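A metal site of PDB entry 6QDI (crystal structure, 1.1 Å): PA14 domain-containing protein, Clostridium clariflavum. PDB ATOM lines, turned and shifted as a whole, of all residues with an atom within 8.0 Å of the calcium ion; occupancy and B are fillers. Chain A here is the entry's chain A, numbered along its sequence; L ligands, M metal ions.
The calcium ion is bound by O of Gly 268 (2.3 Å), O of Ala 270 (2.3 Å), OD1 of Asp 221 (2.4 Å), OD2 of Asp 222 (2.4 Å), OD1 of Asn 266 (2.4 Å), O1 of the ligand (2.5 Å) and O2 of the ligand (2.6 Å).
The calcium ion has seven donor atoms within binding distance.
C of Leu 269 touches the calcium ion (3.97 Å).
Of the 21 residues printed, 6 come within 4 Å of the calcium ion.
Along chain A the residues within 4 Å of the calcium ion span positions 221 to 270.
The nearest printed residue that does not touch the calcium ion is Thr 267 (4.4 Å).
O of Asp 221 sits at hydrogen-bond distance from OH of Tyr 264 (2.6 Å).
The backbone carbonyl oxygen (O) of Ser 272 is in hydrogen-bond range of the backbone NH (N) of Asp 221.
The side-chain hydroxyl (OG1) of Thr 267 is in hydrogen-bond range of the side-chain carboxylate (OD1) of Asp 222 (2.6 Å).
N of Asp 222 is in hydrogen-bond range of O of Arg 265, at 3.0 Å.
N of Glu 241 lies within hydrogen-bond range of O of Asp 222 (3.2 Å).
N of Ser 240 sits at hydrogen-bond distance from O of Asp 222, at 3.1 Å.
ND2 of Asn 266 lies within hydrogen-bond range of O of Leu 269 (3.0 Å).
N of Asn 266 is in hydrogen-bond range of O of Phe 198 (2.9 Å).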
ATOM      1  N   GLY A 184      13.575  -0.515   2.895  1.00  0.00           N
ATOM      2  CA  GLY A 184      12.300  -0.417   3.601  1.00  0.00           C
ATOM      3  C   GLY A 184      11.315  -1.359   2.964  1.00  0.00           C
ATOM      4  O   GLY A 184      11.614  -2.548   2.808  1.00  0.00           O
ATOM      5  N   VAL A 185      10.167  -0.857   2.592  1.00  0.00           N
ATOM      6  CA  VAL A 185       9.145  -1.649   1.925  1.00  0.00           C
ATOM      7  C   VAL A 185       9.184  -1.468   0.401  1.00  0.00           C
ATOM      8  O   VAL A 185       8.307  -1.995  -0.307  1.00  0.00           O
ATOM      9  CB  VAL A 185       7.743  -1.434   2.524  1.00  0.00           C
ATOM     10  CG1 VAL A 185       7.721  -1.933   3.943  1.00  0.00           C
ATOM     11  CG2 VAL A 185       7.294   0.005   2.392  1.00  0.00           C
ATOM     12  N   GLN A 196       6.599  -6.172  -1.572  1.00  0.00           N
ATOM     13  CA  GLN A 196       7.413  -6.748  -0.502  1.00  0.00           C
ATOM     14  C   GLN A 196       7.663  -8.235  -0.644  1.00  0.00           C
ATOM     15  O   GLN A 196       8.054  -8.865   0.283  1.00  0.00           O
ATOM     16  CB  GLN A 196       6.914  -6.409   0.919  1.00  0.00           C
ATOM     17  CG  GLN A 196       6.770  -4.902   1.185  1.00  0.00           C
ATOM     18  CD  GLN A 196       5.507  -4.332   0.576  1.00  0.00           C
ATOM     19  OE1 GLN A 196       4.409  -4.849   0.785  1.00  0.00           O
ATOM     20  NE2 GLN A 196       5.635  -3.214  -0.085  1.00  0.00           N
ATOM     21  N   LYS A 197       7.481  -8.775  -1.852  1.00  0.00           N
ATOM     22  CA  LYS A 197       7.681 -10.180  -2.108  1.00  0.00           C
ATOM     23  C   LYS A 197       8.486 -10.259  -3.393  1.00  0.00           C
ATOM     24  O   LYS A 197       7.928 -10.197  -4.518  1.00  0.00           O
ATOM     25  CB  LYS A 197       6.332 -10.876  -2.269  1.00  0.00           C
ATOM     26  CG  LYS A 197       5.537 -10.912  -0.997  1.00  0.00           C
ATOM     27  CD  LYS A 197       4.188 -11.573  -1.212  1.00  0.00           C
ATOM     28  CE  LYS A 197       3.257 -10.654  -1.968  1.00  0.00           C
ATOM     29  N   PHE A 198       9.815 -10.375  -3.259  1.00  0.00           N
ATOM     30  CA  PHE A 198      10.698 -10.294  -4.417  1.00  0.00           C
ATOM     31  C   PHE A 198      12.006 -10.951  -4.020  1.00  0.00           C
ATOM     32  O   PHE A 198      12.223 -11.258  -2.857  1.00  0.00           O
ATOM     33  CB  PHE A 198      10.865  -8.853  -4.898  1.00  0.00           C
ATOM     34  CG  PHE A 198      11.466  -7.926  -3.879  1.00  0.00           C
ATOM     35  CD1 PHE A 198      12.829  -7.884  -3.648  1.00  0.00           C
ATOM     36  CD2 PHE A 198      10.661  -7.061  -3.127  1.00  0.00           C
ATOM     37  CE1 PHE A 198      13.361  -7.030  -2.659  1.00  0.00           C
ATOM     38  CE2 PHE A 198      11.215  -6.213  -2.188  1.00  0.00           C
ATOM     39  CZ  PHE A 198      12.545  -6.183  -1.955  1.00  0.00           C
ATOM     40  N   TYR A 220      20.407  -9.978   6.734  1.00  0.00           N
ATOM     41  CA  TYR A 220      19.276 -10.127   5.809  1.00  0.00           C
ATOM     42  C   TYR A 220      17.941  -9.917   6.518  1.00  0.00           C
ATOM     43  O   TYR A 220      17.789 -10.240   7.716  1.00  0.00           O
ATOM     44  CB  TYR A 220      19.284 -11.536   5.137  1.00  0.00           C
ATOM     45  CG  TYR A 220      19.311 -12.687   6.120  1.00  0.00           C
ATOM     46  CD1 TYR A 220      20.490 -13.190   6.609  1.00  0.00           C
ATOM     47  CD2 TYR A 220      18.133 -13.262   6.619  1.00  0.00           C
ATOM     48  CE1 TYR A 220      20.528 -14.184   7.582  1.00  0.00           C
ATOM     49  CE2 TYR A 220      18.183 -14.291   7.552  1.00  0.00           C
ATOM     50  CZ  TYR A 220      19.373 -14.718   8.058  1.00  0.00           C
ATOM     51  OH  TYR A 220      19.467 -15.710   9.012  1.00  0.00           O
ATOM     52  N   ASP A 221      16.998  -9.447   5.710  1.00  0.00           N
ATOM     53  CA  ASP A 221      15.581  -9.445   6.084  1.00  0.00           C
ATOM     54  C   ASP A 221      14.908  -9.790   4.743  1.00  0.00           C
ATOM     55  O   ASP A 221      14.869  -8.919   3.874  1.00  0.00           O
ATOM     56  CB  ASP A 221      15.131  -8.069   6.552  1.00  0.00           C
ATOM     57  CG  ASP A 221      13.639  -7.974   6.746  1.00  0.00           C
ATOM     58  OD1 ASP A 221      12.906  -8.901   6.281  1.00  0.00           O
ATOM     59  OD2 ASP A 221      13.191  -6.974   7.349  1.00  0.00           O
ATOM     60  N   ASP A 222      14.486 -11.049   4.493  1.00  0.00           N
ATOM     61  CA  ASP A 222      14.253 -12.094   5.464  1.00  0.00           C
ATOM     62  C   ASP A 222      14.696 -13.504   5.080  1.00  0.00           C
ATOM     63  O   ASP A 222      14.460 -14.411   5.858  1.00  0.00           O
ATOM     64  CB  ASP A 222      12.787 -12.085   5.950  1.00  0.00           C
ATOM     65  CG  ASP A 222      11.823 -12.175   4.832  1.00  0.00           C
ATOM     66  OD1 ASP A 222      11.661 -13.301   4.272  1.00  0.00           O
ATOM     67  OD2 ASP A 222      11.190 -11.154   4.441  1.00  0.00           O
ATOM     68  N   GLY A 223      15.359 -13.672   3.956  1.00  0.00           N
ATOM     69  CA  GLY A 223      16.023 -14.928   3.656  1.00  0.00           C
ATOM     70  C   GLY A 223      17.238 -14.691   2.784  1.00  0.00           C
ATOM     71  O   GLY A 223      17.252 -13.736   1.984  1.00  0.00           O
ATOM     72  N   SER A 240      13.044 -16.759   7.274  1.00  0.00           N
ATOM     73  CA  SER A 240      11.858 -15.890   7.496  1.00  0.00           C
ATOM     74  C   SER A 240      12.113 -15.111   8.774  1.00  0.00           C
ATOM     75  O   SER A 240      11.323 -15.215   9.752  1.00  0.00           O
ATOM     76  CB  SER A 240      10.583 -16.768   7.565  1.00  0.00           C
ATOM     77  OG  SER A 240       9.382 -16.012   7.592  1.00  0.00           O
ATOM     78  N   GLU A 241      13.221 -14.389   8.835  1.00  0.00           N
ATOM     79  CA  GLU A 241      13.589 -13.608  10.021  1.00  0.00           C
ATOM     80  C   GLU A 241      14.525 -12.471   9.602  1.00  0.00           C
ATOM     81  O   GLU A 241      15.109 -12.436   8.513  1.00  0.00           O
ATOM     82  CB  GLU A 241      14.400 -14.507  11.009  1.00  0.00           C
ATOM     83  CG  GLU A 241      15.734 -15.029  10.425  1.00  0.00           C
ATOM     84  CD  GLU A 241      16.588 -15.883  11.367  1.00  0.00           C
ATOM     85  OE1 GLU A 241      16.243 -16.016  12.570  1.00  0.00           O
ATOM     86  OE2 GLU A 241      17.646 -16.409  10.880  1.00  0.00           O
ATOM     87  N   ILE A 242      14.738 -11.547  10.525  1.00  0.00           N
ATOM     88  CA  ILE A 242      15.767 -10.512  10.385  1.00  0.00           C
ATOM     89  C   ILE A 242      16.932 -10.980  11.210  1.00  0.00           C
ATOM     90  O   ILE A 242      16.797 -11.131  12.415  1.00  0.00           O
ATOM     91  CB  ILE A 242      15.277  -9.150  10.919  1.00  0.00           C
ATOM     92  CG1 ILE A 242      13.953  -8.750  10.238  1.00  0.00           C
ATOM     93  CG2 ILE A 242      16.362  -8.072  10.725  1.00  0.00           C
ATOM     94  CD1 ILE A 242      13.215  -7.620  10.915  1.00  0.00           C
ATOM     95  N   TYR A 264      18.877 -13.766  -2.253  1.00  0.00           N
ATOM     96  CA  TYR A 264      18.197 -12.937  -1.264  1.00  0.00           C
ATOM     97  C   TYR A 264      16.714 -12.902  -1.545  1.00  0.00           C
ATOM     98  O   TYR A 264      16.311 -12.880  -2.703  1.00  0.00           O
ATOM     99  CB  TYR A 264      18.794 -11.497  -1.341  1.00  0.00           C
ATOM    100  CG  TYR A 264      17.889 -10.538  -0.624  1.00  0.00           C
ATOM    101  CD1 TYR A 264      17.793 -10.543   0.776  1.00  0.00           C
ATOM    102  CD2 TYR A 264      16.990  -9.783  -1.324  1.00  0.00           C
ATOM    103  CE1 TYR A 264      16.819  -9.805   1.407  1.00  0.00           C
ATOM    104  CE2 TYR A 264      16.007  -9.074  -0.685  1.00  0.00           C
ATOM    105  CZ  TYR A 264      15.914  -9.101   0.691  1.00  0.00           C
ATOM    106  OH  TYR A 264      14.900  -8.376   1.303  1.00  0.00           O
ATOM    107  N   ARG A 265      15.885 -12.832  -0.478  1.00  0.00           N
ATOM    108  CA  ARG A 265      14.474 -12.609  -0.682  1.00  0.00           C
ATOM    109  C   ARG A 265      13.871 -11.751   0.427  1.00  0.00           C
ATOM    110  O   ARG A 265      14.285 -11.805   1.596  1.00  0.00           O
ATOM    111  CB  ARG A 265      13.708 -13.931  -0.733  1.00  0.00           C
ATOM    112  CG  ARG A 265      13.669 -14.660   0.571  1.00  0.00           C
ATOM    113  CD  ARG A 265      13.451 -16.120   0.479  1.00  0.00           C
ATOM    114  NE  ARG A 265      12.331 -16.513  -0.324  1.00  0.00           N
ATOM    115  CZ  ARG A 265      11.748 -17.706  -0.212  1.00  0.00           C
ATOM    116  NH1 ARG A 265      12.107 -18.556   0.725  1.00  0.00           N
ATOM    117  NH2 ARG A 265      10.762 -18.000  -1.031  1.00  0.00           N
ATOM    118  N   ASN A 266      12.850 -11.010   0.011  1.00  0.00           N
ATOM    119  CA  ASN A 266      11.881 -10.405   0.939  1.00  0.00           C
ATOM    120  C   ASN A 266      10.584 -11.170   0.728  1.00  0.00           C
ATOM    121  O   ASN A 266      10.137 -11.326  -0.405  1.00  0.00           O
ATOM    122  CB  ASN A 266      11.660  -8.929   0.654  1.00  0.00           C
ATOM    123  CG  ASN A 266      10.875  -8.240   1.770  1.00  0.00           C
ATOM    124  OD1 ASN A 266      10.548  -8.848   2.783  1.00  0.00           O
ATOM    125  ND2 ASN A 266      10.572  -6.967   1.592  1.00  0.00           N
ATOM    126  N   THR A 267       9.970 -11.624   1.817  1.00  0.00           N
ATOM    127  CA  THR A 267       8.694 -12.317   1.763  1.00  0.00           C
ATOM    128  C   THR A 267       7.546 -11.514   2.376  1.00  0.00           C
ATOM    129  O   THR A 267       6.424 -11.991   2.403  1.00  0.00           O
ATOM    130  CB  THR A 267       8.760 -13.729   2.380  1.00  0.00           C
ATOM    131  OG1 THR A 267       9.091 -13.628   3.759  1.00  0.00           O
ATOM    132  CG2 THR A 267       9.735 -14.630   1.645  1.00  0.00           C
ATOM    133  N   GLY A 268       7.854 -10.322   2.887  1.00  0.00           N
ATOM    134  CA  GLY A 268       6.826  -9.462   3.434  1.00  0.00           C
ATOM    135  C   GLY A 268       7.479  -8.383   4.320  1.00  0.00           C
ATOM    136  O   GLY A 268       8.534  -8.576   4.914  1.00  0.00           O
ATOM    137  N   LEU A 269       6.776  -7.261   4.464  1.00  0.00           N
ATOM    138  CA  LEU A 269       7.233  -6.128   5.242  1.00  0.00           C
ATOM    139  C   LEU A 269       8.590  -5.657   4.687  1.00  0.00           C
ATOM    140  O   LEU A 269       8.738  -5.544   3.474  1.00  0.00           O
ATOM    141  CB  LEU A 269       7.262  -6.430   6.755  1.00  0.00           C
ATOM    142  CG  LEU A 269       6.004  -7.023   7.373  1.00  0.00           C
ATOM    143  CD1 LEU A 269       6.216  -7.165   8.892  1.00  0.00           C
ATOM    144  CD2 LEU A 269       4.815  -6.142   7.117  1.00  0.00           C
ATOM    145  N   ALA A 270       9.524  -5.256   5.555  1.00  0.00           N
ATOM    146  CA  ALA A 270      10.723  -4.628   5.070  1.00  0.00           C
ATOM    147  C   ALA A 270      11.702  -5.594   4.431  1.00  0.00           C
ATOM    148  O   ALA A 270      11.590  -6.825   4.592  1.00  0.00           O
ATOM    149  CB  ALA A 270      11.378  -3.857   6.227  1.00  0.00           C
ATOM    150  N   GLY A 271      12.671  -5.040   3.720  1.00  0.00           N
ATOM    151  CA  GLY A 271      13.702  -5.836   3.048  1.00  0.00           C
ATOM    152  C   GLY A 271      15.053  -5.155   3.119  1.00  0.00           C
ATOM    153  O   GLY A 271      15.158  -3.931   2.918  1.00  0.00           O
ATOM    154  N   SER A 272      16.086  -5.955   3.375  1.00  0.00           N
ATOM    155  CA  SER A 272      17.460  -5.426   3.477  1.00  0.00           C
ATOM    156  C   SER A 272      18.428  -6.593   3.347  1.00  0.00           C
ATOM    157  O   SER A 272      18.079  -7.747   3.665  1.00  0.00           O
ATOM    158  CB  SER A 272      17.656  -4.674   4.815  1.00  0.00           C
ATOM    159  OG  SER A 272      17.390  -5.535   5.924  1.00  0.00           O
HETATM  160  C1  LIG L   1       9.267  -9.464   8.077  1.00  0.00           C
HETATM  161  O1  LIG L   1       9.933 -10.248   7.073  1.00  0.00           O
HETATM  162  C2  LIG L   1      10.216  -8.314   8.454  1.00  0.00           C
HETATM  163  O2  LIG L   1      10.525  -7.510   7.313  1.00  0.00           O
HETATM  164 CA    CA M   1      10.801  -8.918   5.196  1.00  0.00          CA
